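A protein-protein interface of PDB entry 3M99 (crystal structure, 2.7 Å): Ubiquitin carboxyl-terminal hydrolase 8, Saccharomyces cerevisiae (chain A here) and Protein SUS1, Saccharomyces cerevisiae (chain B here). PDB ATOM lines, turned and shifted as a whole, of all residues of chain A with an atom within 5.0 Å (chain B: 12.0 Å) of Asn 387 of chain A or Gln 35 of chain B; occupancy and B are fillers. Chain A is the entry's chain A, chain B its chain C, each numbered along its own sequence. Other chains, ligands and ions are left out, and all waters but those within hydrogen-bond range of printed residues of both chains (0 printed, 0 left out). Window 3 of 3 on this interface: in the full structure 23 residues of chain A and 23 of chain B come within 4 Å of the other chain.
The side-chain carboxylate of Asp 408 of chain A lies close to the side-chain carboxylate of Glu 28 of chain B, 3.4 Å away.
The side-chain amide nitrogen of Asn 387 of chain A lies close to the side-chain amide nitrogen of Gln 35 of chain B, at 3.0 Å.
The side-chain hydroxyl (OH) of Tyr 385 of chain A lies within hydrogen-bond range of the side-chain carboxylate (OD1) of Asp 40 of chain B (2.8 Å).
The side-chain carboxylate (OD1) of Asp 408 of chain A lies within hydrogen-bond range of the side-chain amide nitrogen (ND2) of Asn 387 of chain A, at 3.3 Å.
NZ of Lys 389 of chain A is in salt-bridge range of OD1 of Asp 408 of chain A.
The side-chain amide oxygen (OD1) of Asn 387 of chain A lies close to the backbone carbonyl oxygen (O) of Ile 409 of chain A (3.1 Å).
N of Lys 389 of chain A lies within hydrogen-bond range of OD1 of Asn 387 of chain A.
The side-chain hydroxyl (OH) of Tyr 317 of chain A sits at hydrogen-bond distance from the backbone NH (N) of Asn 387 of chain A, 3.0 Å away.
NH1 of Arg 32 of chain B lies within salt-bridge range of OE1 of Glu 28 of chain B, 2.9 Å away.
Among the printed residues, merely in contact across the chains: Ile 410 of chain A with Gln 35 of chain B (3.2 Å), Tyr 385 of chain A with Leu 34 of chain B (3.4 Å) and Ile 410 of chain A with Ala 31 of chain B (3.95 Å).
Tyr 385 of chain A touches just these residues of chain B: Leu 34 and Asp 40.
Asn 387 of chain A touches just one residue of chain B: Gln 35 (3.0 Å).
No residue of chain B comes within 4 Å of Met 388 of chain A.
Lys 389 of chain A touches none of the printed residues of chain B.
Of chain B, only Glu 28 comes within 4 Å of Asp 408 of chain A.
No residue of chain B comes within 4 Å of Ile 409 of chain A.
Printed residues of chain A within 4 Å of Glu 28 of chain B: Asp 408 (3.4 Å).
Of the printed residues of chain A, Ala 31 of chain B touches Ile 410.
Of the printed residues of chain A, Leu 34 of chain B touches Tyr 385.
Of the printed residues of chain A, Gln 35 of chain B touches Asn 387 and Ile 410.
Of the printed residues of chain A, Asp 40 of chain B touches Tyr 385.
Val 73 of chain B touches none of the printed residues of chain A.
Thr 77 of chain B touches none of the printed residues of chain A.
The nearest residue of chain B that does not touch Asn 387 of chain A is Ala 31 of chain B (6.6 Å).
The nearest printed residue of chain A that does not touch Leu 34 of chain B is Ile 410 of chain A (4.3 Å).
Of the 25 printed residues of chain B, 5 touch a printed residue of chain A.
Printed residues of chain B that touch a printed residue of chain A: Glu 28, Ala 31, Leu 34, Gln 35 and Asp 40.
Hydrophobic or aromatic side chains of chain B within 4 Å of the printed part of chain A: Ala 31 and Leu 34.
Of the 11 printed residues of chain A, 4 touch a printed residue of chain B.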
ATOM      1  N   TYR A 317      -2.450 -11.743  -9.121  1.00  0.00           N
ATOM      2  CA  TYR A 317      -1.996 -13.093  -8.826  1.00  0.00           C
ATOM      3  C   TYR A 317      -0.478 -13.110  -8.685  1.00  0.00           C
ATOM      4  O   TYR A 317       0.073 -13.913  -7.932  1.00  0.00           O
ATOM      5  CB  TYR A 317      -2.475 -14.095  -9.881  1.00  0.00           C
ATOM      6  CG  TYR A 317      -3.922 -14.534  -9.710  1.00  0.00           C
ATOM      7  CD1 TYR A 317      -4.937 -13.956 -10.459  1.00  0.00           C
ATOM      8  CD2 TYR A 317      -4.268 -15.529  -8.802  1.00  0.00           C
ATOM      9  CE1 TYR A 317      -6.245 -14.350 -10.308  1.00  0.00           C
ATOM     10  CE2 TYR A 317      -5.577 -15.931  -8.647  1.00  0.00           C
ATOM     11  CZ  TYR A 317      -6.561 -15.336  -9.401  1.00  0.00           C
ATOM     12  OH  TYR A 317      -7.876 -15.726  -9.254  1.00  0.00           O
ATOM     13  N   TYR A 385     -13.588 -12.146 -10.016  1.00  0.00           N
ATOM     14  CA  TYR A 385     -13.652 -13.241  -9.043  1.00  0.00           C
ATOM     15  C   TYR A 385     -12.263 -13.796  -8.752  1.00  0.00           C
ATOM     16  O   TYR A 385     -11.496 -14.094  -9.671  1.00  0.00           O
ATOM     17  CB  TYR A 385     -14.568 -14.373  -9.516  1.00  0.00           C
ATOM     18  CG  TYR A 385     -16.022 -13.988  -9.606  1.00  0.00           C
ATOM     19  CD1 TYR A 385     -16.604 -13.702 -10.830  1.00  0.00           C
ATOM     20  CD2 TYR A 385     -16.809 -13.902  -8.468  1.00  0.00           C
ATOM     21  CE1 TYR A 385     -17.927 -13.343 -10.918  1.00  0.00           C
ATOM     22  CE2 TYR A 385     -18.132 -13.547  -8.544  1.00  0.00           C
ATOM     23  CZ  TYR A 385     -18.689 -13.267  -9.772  1.00  0.00           C
ATOM     24  OH  TYR A 385     -20.017 -12.911  -9.854  1.00  0.00           O
ATOM     25  N   LEU A 386     -11.951 -13.947  -7.469  1.00  0.00           N
ATOM     26  CA  LEU A 386     -10.603 -14.297  -7.048  1.00  0.00           C
ATOM     27  C   LEU A 386     -10.533 -15.689  -6.456  1.00  0.00           C
ATOM     28  O   LEU A 386     -11.283 -16.012  -5.540  1.00  0.00           O
ATOM     29  CB  LEU A 386     -10.108 -13.302  -6.004  1.00  0.00           C
ATOM     30  CG  LEU A 386      -8.781 -13.683  -5.347  1.00  0.00           C
ATOM     31  CD1 LEU A 386      -7.635 -13.510  -6.332  1.00  0.00           C
ATOM     32  CD2 LEU A 386      -8.553 -12.852  -4.099  1.00  0.00           C
ATOM     33  N   ASN A 387      -9.616 -16.507  -6.963  1.00  0.00           N
ATOM     34  CA  ASN A 387      -9.387 -17.833  -6.398  1.00  0.00           C
ATOM     35  C   ASN A 387      -8.149 -17.846  -5.498  1.00  0.00           C
ATOM     36  O   ASN A 387      -7.133 -17.243  -5.830  1.00  0.00           O
ATOM     37  CB  ASN A 387      -9.242 -18.865  -7.513  1.00  0.00           C
ATOM     38  CG  ASN A 387      -9.617 -20.264  -7.068  1.00  0.00           C
ATOM     39  OD1 ASN A 387      -9.490 -20.616  -5.893  1.00  0.00           O
ATOM     40  ND2 ASN A 387     -10.083 -21.073  -8.013  1.00  0.00           N
ATOM     41  N   MET A 388      -8.237 -18.544  -4.369  1.00  0.00           N
ATOM     42  CA  MET A 388      -7.173 -18.555  -3.375  1.00  0.00           C
ATOM     43  C   MET A 388      -6.629 -19.959  -3.152  1.00  0.00           C
ATOM     44  O   MET A 388      -5.830 -20.185  -2.238  1.00  0.00           O
ATOM     45  CB  MET A 388      -7.701 -18.022  -2.046  1.00  0.00           C
ATOM     46  CG  MET A 388      -8.146 -16.569  -2.070  1.00  0.00           C
ATOM     47  SD  MET A 388      -6.802 -15.401  -1.760  1.00  0.00           S
ATOM     48  CE  MET A 388      -6.142 -15.213  -3.410  1.00  0.00           C
ATOM     49  N   LYS A 389      -7.071 -20.904  -3.974  1.00  0.00           N
ATOM     50  CA  LYS A 389      -6.673 -22.296  -3.795  1.00  0.00           C
ATOM     51  C   LYS A 389      -5.155 -22.453  -3.822  1.00  0.00           C
ATOM     52  O   LYS A 389      -4.611 -23.367  -3.204  1.00  0.00           O
ATOM     53  CB  LYS A 389      -7.335 -23.207  -4.835  1.00  0.00           C
ATOM     54  CG  LYS A 389      -6.943 -22.915  -6.263  1.00  0.00           C
ATOM     55  CD  LYS A 389      -7.266 -24.088  -7.173  1.00  0.00           C
ATOM     56  CE  LYS A 389      -6.746 -23.848  -8.588  1.00  0.00           C
ATOM     57  NZ  LYS A 389      -7.262 -24.847  -9.583  1.00  0.00           N
ATOM     58  N   TYR A 391      -2.876 -20.291  -2.596  1.00  0.00           N
ATOM     59  CA  TYR A 391      -2.136 -19.567  -1.560  1.00  0.00           C
ATOM     60  C   TYR A 391      -2.331 -20.124  -0.156  1.00  0.00           C
ATOM     61  O   TYR A 391      -1.799 -19.585   0.813  1.00  0.00           O
ATOM     62  CB  TYR A 391      -2.439 -18.069  -1.637  1.00  0.00           C
ATOM     63  CG  TYR A 391      -2.323 -17.603  -3.057  1.00  0.00           C
ATOM     64  CD1 TYR A 391      -3.436 -17.199  -3.776  1.00  0.00           C
ATOM     65  CD2 TYR A 391      -1.102 -17.647  -3.709  1.00  0.00           C
ATOM     66  CE1 TYR A 391      -3.324 -16.809  -5.094  1.00  0.00           C
ATOM     67  CE2 TYR A 391      -0.980 -17.261  -5.021  1.00  0.00           C
ATOM     68  CZ  TYR A 391      -2.091 -16.844  -5.709  1.00  0.00           C
ATOM     69  OH  TYR A 391      -1.947 -16.463  -7.019  1.00  0.00           O
ATOM     70  N   ASP A 408     -10.950 -25.370  -5.008  1.00  0.00           N
ATOM     71  CA  ASP A 408     -11.309 -24.022  -5.407  1.00  0.00           C
ATOM     72  C   ASP A 408     -12.002 -23.277  -4.266  1.00  0.00           C
ATOM     73  O   ASP A 408     -12.976 -23.762  -3.696  1.00  0.00           O
ATOM     74  CB  ASP A 408     -12.245 -24.083  -6.618  1.00  0.00           C
ATOM     75  CG  ASP A 408     -11.629 -24.814  -7.801  1.00  0.00           C
ATOM     76  OD1 ASP A 408     -10.660 -24.294  -8.399  1.00  0.00           O
ATOM     77  OD2 ASP A 408     -12.122 -25.908  -8.145  1.00  0.00           O
ATOM     78  N   ILE A 409     -11.481 -22.104  -3.926  1.00  0.00           N
ATOM     79  CA  ILE A 409     -12.112 -21.233  -2.944  1.00  0.00           C
ATOM     80  C   ILE A 409     -12.197 -19.865  -3.592  1.00  0.00           C
ATOM     81  O   ILE A 409     -11.188 -19.182  -3.726  1.00  0.00           O
ATOM     82  CB  ILE A 409     -11.289 -21.131  -1.635  1.00  0.00           C
ATOM     83  CG1 ILE A 409     -10.780 -22.501  -1.206  1.00  0.00           C
ATOM     84  CG2 ILE A 409     -12.119 -20.514  -0.517  1.00  0.00           C
ATOM     85  CD1 ILE A 409     -10.285 -22.535   0.209  1.00  0.00           C
ATOM     86  N   ILE A 410     -13.398 -19.474  -4.011  1.00  0.00           N
ATOM     87  CA  ILE A 410     -13.578 -18.291  -4.851  1.00  0.00           C
ATOM     88  C   ILE A 410     -14.264 -17.141  -4.116  1.00  0.00           C
ATOM     89  O   ILE A 410     -15.259 -17.342  -3.424  1.00  0.00           O
ATOM     90  CB  ILE A 410     -14.356 -18.640  -6.132  1.00  0.00           C
ATOM     91  CG1 ILE A 410     -13.562 -19.645  -6.970  1.00  0.00           C
ATOM     92  CG2 ILE A 410     -14.639 -17.392  -6.932  1.00  0.00           C
ATOM     93  CD1 ILE A 410     -14.401 -20.481  -7.905  1.00  0.00           C
ATOM     94  N   TYR A 411     -13.707 -15.943  -4.269  1.00  0.00           N
ATOM     95  CA  TYR A 411     -14.204 -14.739  -3.624  1.00  0.00           C
ATOM     96  C   TYR A 411     -14.811 -13.848  -4.683  1.00  0.00           C
ATOM     97  O   TYR A 411     -14.521 -14.008  -5.864  1.00  0.00           O
ATOM     98  CB  TYR A 411     -13.048 -13.984  -2.966  1.00  0.00           C
ATOM     99  CG  TYR A 411     -12.626 -14.511  -1.614  1.00  0.00           C
ATOM    100  CD1 TYR A 411     -11.715 -15.547  -1.506  1.00  0.00           C
ATOM    101  CD2 TYR A 411     -13.138 -13.962  -0.448  1.00  0.00           C
ATOM    102  CE1 TYR A 411     -11.331 -16.022  -0.280  1.00  0.00           C
ATOM    103  CE2 TYR A 411     -12.768 -14.434   0.779  1.00  0.00           C
ATOM    104  CZ  TYR A 411     -11.861 -15.464   0.862  1.00  0.00           C
ATOM    105  OH  TYR A 411     -11.477 -15.942   2.094  1.00  0.00           O
ATOM    106  N   SER B  26     -21.117 -30.978  -9.995  1.00  0.00           N
ATOM    107  CA  SER B  26     -21.902 -29.754  -9.942  1.00  0.00           C
ATOM    108  C   SER B  26     -21.006 -28.589  -9.597  1.00  0.00           C
ATOM    109  O   SER B  26     -21.016 -27.556 -10.273  1.00  0.00           O
ATOM    110  CB  SER B  26     -22.996 -29.860  -8.891  1.00  0.00           C
ATOM    111  OG  SER B  26     -24.173 -30.389  -9.458  1.00  0.00           O
ATOM    112  N   ASN B  27     -20.237 -28.769  -8.527  1.00  0.00           N
ATOM    113  CA  ASN B  27     -19.355 -27.727  -8.024  1.00  0.00           C
ATOM    114  C   ASN B  27     -18.272 -27.356  -9.028  1.00  0.00           C
ATOM    115  O   ASN B  27     -18.092 -26.184  -9.349  1.00  0.00           O
ATOM    116  CB  ASN B  27     -18.755 -28.147  -6.686  1.00  0.00           C
ATOM    117  CG  ASN B  27     -19.801 -28.249  -5.589  1.00  0.00           C
ATOM    118  OD1 ASN B  27     -20.933 -27.782  -5.748  1.00  0.00           O
ATOM    119  ND2 ASN B  27     -19.427 -28.857  -4.467  1.00  0.00           N
ATOM    120  N   GLU B  28     -17.558 -28.354  -9.534  1.00  0.00           N
ATOM    121  CA  GLU B  28     -16.573 -28.106 -10.575  1.00  0.00           C
ATOM    122  C   GLU B  28     -17.177 -27.282 -11.703  1.00  0.00           C
ATOM    123  O   GLU B  28     -16.602 -26.279 -12.116  1.00  0.00           O
ATOM    124  CB  GLU B  28     -16.001 -29.418 -11.106  1.00  0.00           C
ATOM    125  CG  GLU B  28     -14.858 -29.967 -10.261  1.00  0.00           C
ATOM    126  CD  GLU B  28     -13.585 -29.136 -10.392  1.00  0.00           C
ATOM    127  OE1 GLU B  28     -13.286 -28.665 -11.513  1.00  0.00           O
ATOM    128  OE2 GLU B  28     -12.877 -28.962  -9.377  1.00  0.00           O
ATOM    129  N   LEU B  29     -18.344 -27.700 -12.189  1.00  0.00           N
ATOM    130  CA  LEU B  29     -19.052 -26.956 -13.227  1.00  0.00           C
ATOM    131  C   LEU B  29     -19.499 -25.575 -12.746  1.00  0.00           C
ATOM    132  O   LEU B  29     -19.284 -24.580 -13.432  1.00  0.00           O
ATOM    133  CB  LEU B  29     -20.249 -27.755 -13.750  1.00  0.00           C
ATOM    134  CG  LEU B  29     -21.206 -27.092 -14.754  1.00  0.00           C
ATOM    135  CD1 LEU B  29     -20.472 -26.437 -15.915  1.00  0.00           C
ATOM    136  CD2 LEU B  29     -22.207 -28.109 -15.274  1.00  0.00           C
ATOM    137  N   LYS B  30     -20.126 -25.511 -11.574  1.00  0.00           N
ATOM    138  CA  LYS B  30     -20.534 -24.224 -11.016  1.00  0.00           C
ATOM    139  C   LYS B  30     -19.362 -23.251 -11.039  1.00  0.00           C
ATOM    140  O   LYS B  30     -19.472 -22.137 -11.554  1.00  0.00           O
ATOM    141  CB  LYS B  30     -21.034 -24.375  -9.576  1.00  0.00           C
ATOM    142  CG  LYS B  30     -22.460 -24.887  -9.421  1.00  0.00           C
ATOM    143  CD  LYS B  30     -22.937 -24.713  -7.978  1.00  0.00           C
ATOM    144  CE  LYS B  30     -24.314 -25.334  -7.742  1.00  0.00           C
ATOM    145  NZ  LYS B  30     -24.290 -26.834  -7.739  1.00  0.00           N
ATOM    146  N   ALA B  31     -18.238 -23.696 -10.476  1.00  0.00           N
ATOM    147  CA  ALA B  31     -17.029 -22.882 -10.345  1.00  0.00           C
ATOM    148  C   ALA B  31     -16.534 -22.352 -11.686  1.00  0.00           C
ATOM    149  O   ALA B  31     -16.362 -21.153 -11.853  1.00  0.00           O
ATOM    150  CB  ALA B  31     -15.933 -23.677  -9.652  1.00  0.00           C
ATOM    151  N   ARG B  32     -16.303 -23.252 -12.634  1.00  0.00           N
ATOM    152  CA  ARG B  32     -15.899 -22.863 -13.977  1.00  0.00           C
ATOM    153  C   ARG B  32     -16.841 -21.833 -14.597  1.00  0.00           C
ATOM    154  O   ARG B  32     -16.411 -20.936 -15.327  1.00  0.00           O
ATOM    155  CB  ARG B  32     -15.815 -24.089 -14.878  1.00  0.00           C
ATOM    156  CG  ARG B  32     -14.561 -24.903 -14.685  1.00  0.00           C
ATOM    157  CD  ARG B  32     -14.484 -26.020 -15.703  1.00  0.00           C
ATOM    158  NE  ARG B  32     -13.107 -26.328 -16.063  1.00  0.00           N
ATOM    159  CZ  ARG B  32     -12.292 -27.069 -15.323  1.00  0.00           C
ATOM    160  NH1 ARG B  32     -12.716 -27.578 -14.173  1.00  0.00           N
ATOM    161  NH2 ARG B  32     -11.051 -27.298 -15.732  1.00  0.00           N
ATOM    162  N   LEU B  33     -18.131 -21.965 -14.313  1.00  0.00           N
ATOM    163  CA  LEU B  33     -19.115 -21.035 -14.848  1.00  0.00           C
ATOM    164  C   LEU B  33     -19.082 -19.692 -14.130  1.00  0.00           C
ATOM    165  O   LEU B  33     -19.303 -18.652 -14.740  1.00  0.00           O
ATOM    166  CB  LEU B  33     -20.517 -21.637 -14.775  1.00  0.00           C
ATOM    167  CG  LEU B  33     -20.831 -22.683 -15.841  1.00  0.00           C
ATOM    168  CD1 LEU B  33     -22.186 -23.339 -15.575  1.00  0.00           C
ATOM    169  CD2 LEU B  33     -20.783 -22.045 -17.225  1.00  0.00           C
ATOM    170  N   LEU B  34     -18.806 -19.721 -12.832  1.00  0.00           N
ATOM    171  CA  LEU B  34     -18.791 -18.500 -12.041  1.00  0.00           C
ATOM    172  C   LEU B  34     -17.589 -17.636 -12.384  1.00  0.00           C
ATOM    173  O   LEU B  34     -17.710 -16.415 -12.464  1.00  0.00           O
ATOM    174  CB  LEU B  34     -18.806 -18.803 -10.544  1.00  0.00           C
ATOM    175  CG  LEU B  34     -18.682 -17.544  -9.687  1.00  0.00           C
ATOM    176  CD1 LEU B  34     -19.770 -16.550 -10.041  1.00  0.00           C
ATOM    177  CD2 LEU B  34     -18.729 -17.875  -8.211  1.00  0.00           C
ATOM    178  N   GLN B  35     -16.438 -18.272 -12.592  1.00  0.00           N
ATOM    179  CA  GLN B  35     -15.197 -17.557 -12.887  1.00  0.00           C
ATOM    180  C   GLN B  35     -15.170 -16.938 -14.286  1.00  0.00           C
ATOM    181  O   GLN B  35     -14.615 -15.857 -14.475  1.00  0.00           O
ATOM    182  CB  GLN B  35     -13.988 -18.473 -12.702  1.00  0.00           C
ATOM    183  CG  GLN B  35     -13.826 -19.008 -11.287  1.00  0.00           C
ATOM    184  CD  GLN B  35     -12.386 -18.966 -10.805  1.00  0.00           C
ATOM    185  OE1 GLN B  35     -11.610 -18.089 -11.204  1.00  0.00           O
ATOM    186  NE2 GLN B  35     -12.022 -19.906  -9.933  1.00  0.00           N
ATOM    187  N   GLU B  36     -15.773 -17.627 -15.256  1.00  0.00           N
ATOM    188  CA  GLU B  36     -15.794 -17.190 -16.655  1.00  0.00           C
ATOM    189  C   GLU B  36     -16.774 -16.050 -16.937  1.00  0.00           C
ATOM    190  O   GLU B  36     -17.045 -15.726 -18.102  1.00  0.00           O
ATOM    191  CB  GLU B  36     -16.170 -18.354 -17.571  1.00  0.00           C
ATOM    192  CG  GLU B  36     -15.166 -19.484 -17.662  1.00  0.00           C
ATOM    193  CD  GLU B  36     -15.646 -20.579 -18.606  1.00  0.00           C
ATOM    194  OE1 GLU B  36     -16.878 -20.793 -18.685  1.00  0.00           O
ATOM    195  OE2 GLU B  36     -14.799 -21.217 -19.272  1.00  0.00           O
ATOM    196  N   GLY B  37     -17.325 -15.461 -15.881  1.00  0.00           N
ATOM    197  CA  GLY B  37     -18.293 -14.384 -16.023  1.00  0.00           C
ATOM    198  C   GLY B  37     -19.565 -14.815 -16.725  1.00  0.00           C
ATOM    199  O   GLY B  37     -20.311 -13.990 -17.262  1.00  0.00           O
ATOM    200  N   TRP B  38     -19.795 -16.122 -16.727  1.00  0.00           N
ATOM    201  CA  TRP B  38     -20.982 -16.702 -17.327  1.00  0.00           C
ATOM    202  C   TRP B  38     -22.204 -16.390 -16.475  1.00  0.00           C
ATOM    203  O   TRP B  38     -23.146 -15.775 -16.957  1.00  0.00           O
ATOM    204  CB  TRP B  38     -20.810 -18.212 -17.495  1.00  0.00           C
ATOM    205  CG  TRP B  38     -21.954 -18.869 -18.182  1.00  0.00           C
ATOM    206  CD1 TRP B  38     -22.171 -18.940 -19.529  1.00  0.00           C
ATOM    207  CD2 TRP B  38     -23.048 -19.555 -17.562  1.00  0.00           C
ATOM    208  NE1 TRP B  38     -23.334 -19.628 -19.784  1.00  0.00           N
ATOM    209  CE2 TRP B  38     -23.891 -20.015 -18.593  1.00  0.00           C
ATOM    210  CE3 TRP B  38     -23.399 -19.823 -16.235  1.00  0.00           C
ATOM    211  CZ2 TRP B  38     -25.059 -20.730 -18.340  1.00  0.00           C
ATOM    212  CZ3 TRP B  38     -24.566 -20.534 -15.986  1.00  0.00           C
ATOM    213  CH2 TRP B  38     -25.377 -20.978 -17.033  1.00  0.00           C
ATOM    214  N   VAL B  39     -22.182 -16.806 -15.211  1.00  0.00           N
ATOM    215  CA  VAL B  39     -23.306 -16.570 -14.309  1.00  0.00           C
ATOM    216  C   VAL B  39     -23.712 -15.111 -14.358  1.00  0.00           C
ATOM    217  O   VAL B  39     -24.890 -14.795 -14.515  1.00  0.00           O
ATOM    218  CB  VAL B  39     -22.981 -16.950 -12.848  1.00  0.00           C
ATOM    219  CG1 VAL B  39     -24.147 -16.593 -11.938  1.00  0.00           C
ATOM    220  CG2 VAL B  39     -22.647 -18.424 -12.739  1.00  0.00           C
ATOM    221  N   ASP B  40     -22.723 -14.229 -14.233  1.00  0.00           N
ATOM    222  CA  ASP B  40     -22.937 -12.786 -14.295  1.00  0.00           C
ATOM    223  C   ASP B  40     -23.552 -12.360 -15.626  1.00  0.00           C
ATOM    224  O   ASP B  40     -24.432 -11.496 -15.664  1.00  0.00           O
ATOM    225  CB  ASP B  40     -21.618 -12.039 -14.104  1.00  0.00           C
ATOM    226  CG  ASP B  40     -20.925 -12.379 -12.791  1.00  0.00           C
ATOM    227  OD1 ASP B  40     -20.988 -13.554 -12.356  1.00  0.00           O
ATOM    228  OD2 ASP B  40     -20.295 -11.465 -12.204  1.00  0.00           O
ATOM    229  N   LYS B  41     -23.074 -12.961 -16.714  1.00  0.00           N
ATOM    230  CA  LYS B  41     -23.510 -12.589 -18.060  1.00  0.00           C
ATOM    231  C   LYS B  41     -24.914 -13.117 -18.367  1.00  0.00           C
ATOM    232  O   LYS B  41     -25.670 -12.505 -19.123  1.00  0.00           O
ATOM    233  CB  LYS B  41     -22.505 -13.081 -19.114  1.00  0.00           C
ATOM    234  CG  LYS B  41     -22.263 -12.085 -20.251  1.00  0.00           C
ATOM    235  CD  LYS B  41     -21.417 -12.676 -21.382  1.00  0.00           C
ATOM    236  CE  LYS B  41     -21.314 -11.695 -22.559  1.00  0.00           C
ATOM    237  NZ  LYS B  41     -20.671 -12.278 -23.777  1.00  0.00           N
ATOM    238  N   VAL B  42     -25.246 -14.259 -17.773  1.00  0.00           N
ATOM    239  CA  VAL B  42     -26.567 -14.851 -17.907  1.00  0.00           C
ATOM    240  C   VAL B  42     -27.555 -14.057 -17.062  1.00  0.00           C
ATOM    241  O   VAL B  42     -28.703 -13.865 -17.453  1.00  0.00           O
ATOM    242  CB  VAL B  42     -26.558 -16.333 -17.473  1.00  0.00           C
ATOM    243  CG1 VAL B  42     -27.968 -16.857 -17.303  1.00  0.00           C
ATOM    244  CG2 VAL B  42     -25.792 -17.179 -18.477  1.00  0.00           C
ATOM    245  N   LYS B  43     -27.101 -13.590 -15.904  1.00  0.00           N
ATOM    246  CA  LYS B  43     -27.931 -12.747 -15.052  1.00  0.00           C
ATOM    247  C   LYS B  43     -28.246 -11.408 -15.740  1.00  0.00           C
ATOM    248  O   LYS B  43     -29.255 -10.769 -15.437  1.00  0.00           O
ATOM    249  CB  LYS B  43     -27.269 -12.526 -13.676  1.00  0.00           C
ATOM    250  CG  LYS B  43     -27.132 -13.800 -12.828  1.00  0.00           C
ATOM    251  CD  LYS B  43     -26.560 -13.547 -11.425  1.00  0.00           C
ATOM    252  CE  LYS B  43     -27.467 -12.642 -10.592  1.00  0.00           C
ATOM    253  NZ  LYS B  43     -26.955 -12.365  -9.211  1.00  0.00           N
ATOM    254  N   MET B  72     -23.918 -19.944 -24.507  1.00  0.00           N
ATOM    255  CA  MET B  72     -22.988 -19.000 -23.890  1.00  0.00           C
ATOM    256  C   MET B  72     -21.846 -19.662 -23.101  1.00  0.00           C
ATOM    257  O   MET B  72     -20.869 -19.003 -22.735  1.00  0.00           O
ATOM    258  CB  MET B  72     -23.760 -18.028 -22.998  1.00  0.00           C
ATOM    259  CG  MET B  72     -23.224 -16.613 -23.010  1.00  0.00           C
ATOM    260  SD  MET B  72     -24.530 -15.418 -22.661  1.00  0.00           S
ATOM    261  CE  MET B  72     -25.408 -15.424 -24.222  1.00  0.00           C
ATOM    262  N   VAL B  73     -21.978 -20.958 -22.838  1.00  0.00           N
ATOM    263  CA  VAL B  73     -20.925 -21.700 -22.154  1.00  0.00           C
ATOM    264  C   VAL B  73     -19.704 -21.853 -23.051  1.00  0.00           C
ATOM    265  O   VAL B  73     -19.818 -22.184 -24.234  1.00  0.00           O
ATOM    266  CB  VAL B  73     -21.397 -23.089 -21.641  1.00  0.00           C
ATOM    267  CG1 VAL B  73     -22.678 -22.939 -20.850  1.00  0.00           C
ATOM    268  CG2 VAL B  73     -21.568 -24.084 -22.793  1.00  0.00           C
ATOM    269  N   SER B  74     -18.531 -21.579 -22.491  1.00  0.00           N
ATOM    270  CA  SER B  74     -17.289 -21.817 -23.220  1.00  0.00           C
ATOM    271  C   SER B  74     -17.205 -23.269 -23.680  1.00  0.00           C
ATOM    272  O   SER B  74     -17.463 -24.193 -22.903  1.00  0.00           O
ATOM    273  CB  SER B  74     -16.069 -21.511 -22.351  1.00  0.00           C
ATOM    274  OG  SER B  74     -15.903 -22.511 -21.359  1.00  0.00           O
ATOM    275  N   SER B  76     -14.726 -24.702 -23.948  1.00  0.00           N
ATOM    276  CA  SER B  76     -13.707 -25.246 -23.063  1.00  0.00           C
ATOM    277  C   SER B  76     -14.354 -25.978 -21.890  1.00  0.00           C
ATOM    278  O   SER B  76     -14.130 -27.174 -21.694  1.00  0.00           O
ATOM    279  CB  SER B  76     -12.794 -24.140 -22.543  1.00  0.00           C
ATOM    280  OG  SER B  76     -11.923 -24.647 -21.547  1.00  0.00           O
ATOM    281  N   THR B  77     -15.159 -25.250 -21.118  1.00  0.00           N
ATOM    282  CA  THR B  77     -15.820 -25.800 -19.933  1.00  0.00           C
ATOM    283  C   THR B  77     -16.626 -27.045 -20.264  1.00  0.00           C
ATOM    284  O   THR B  77     -16.485 -28.076 -19.610  1.00  0.00           O
ATOM    285  CB  THR B  77     -16.776 -24.782 -19.284  1.00  0.00           C
ATOM    286  OG1 THR B  77     -16.033 -23.659 -18.797  1.00  0.00           O
ATOM    287  CG2 THR B  77     -17.518 -25.423 -18.127  1.00  0.00           C
ATOM    288  N   THR B  80     -14.057 -30.076 -20.697  1.00  0.00           N
ATOM    289  CA  THR B  80     -13.428 -30.583 -19.480  1.00  0.00           C
ATOM    290  C   THR B  80     -14.441 -31.265 -18.561  1.00  0.00           C
ATOM    291  O   THR B  80     -14.179 -32.346 -18.036  1.00  0.00           O
ATOM    292  CB  THR B  80     -12.664 -29.480 -18.699  1.00  0.00           C
ATOM    293  OG1 THR B  80     -13.260 -28.205 -18.956  1.00  0.00           O
ATOM    294  CG2 THR B  80     -11.203 -29.430 -19.122  1.00  0.00           C
ATOM    295  N   VAL B  81     -15.601 -30.638 -18.382  1.00  0.00           N
ATOM    296  CA  VAL B  81     -16.618 -31.142 -17.460  1.00  0.00           C
ATOM    297  C   VAL B  81     -17.349 -32.377 -17.986  1.00  0.00           C
ATOM    298  O   VAL B  81     -17.705 -33.267 -17.219  1.00  0.00           O
ATOM    299  CB  VAL B  81     -17.658 -30.064 -17.127  1.00  0.00           C
ATOM    300  CG1 VAL B  81     -18.520 -30.514 -15.969  1.00  0.00           C
ATOM    301  CG2 VAL B  81     -16.970 -28.759 -16.786  1.00  0.00           C
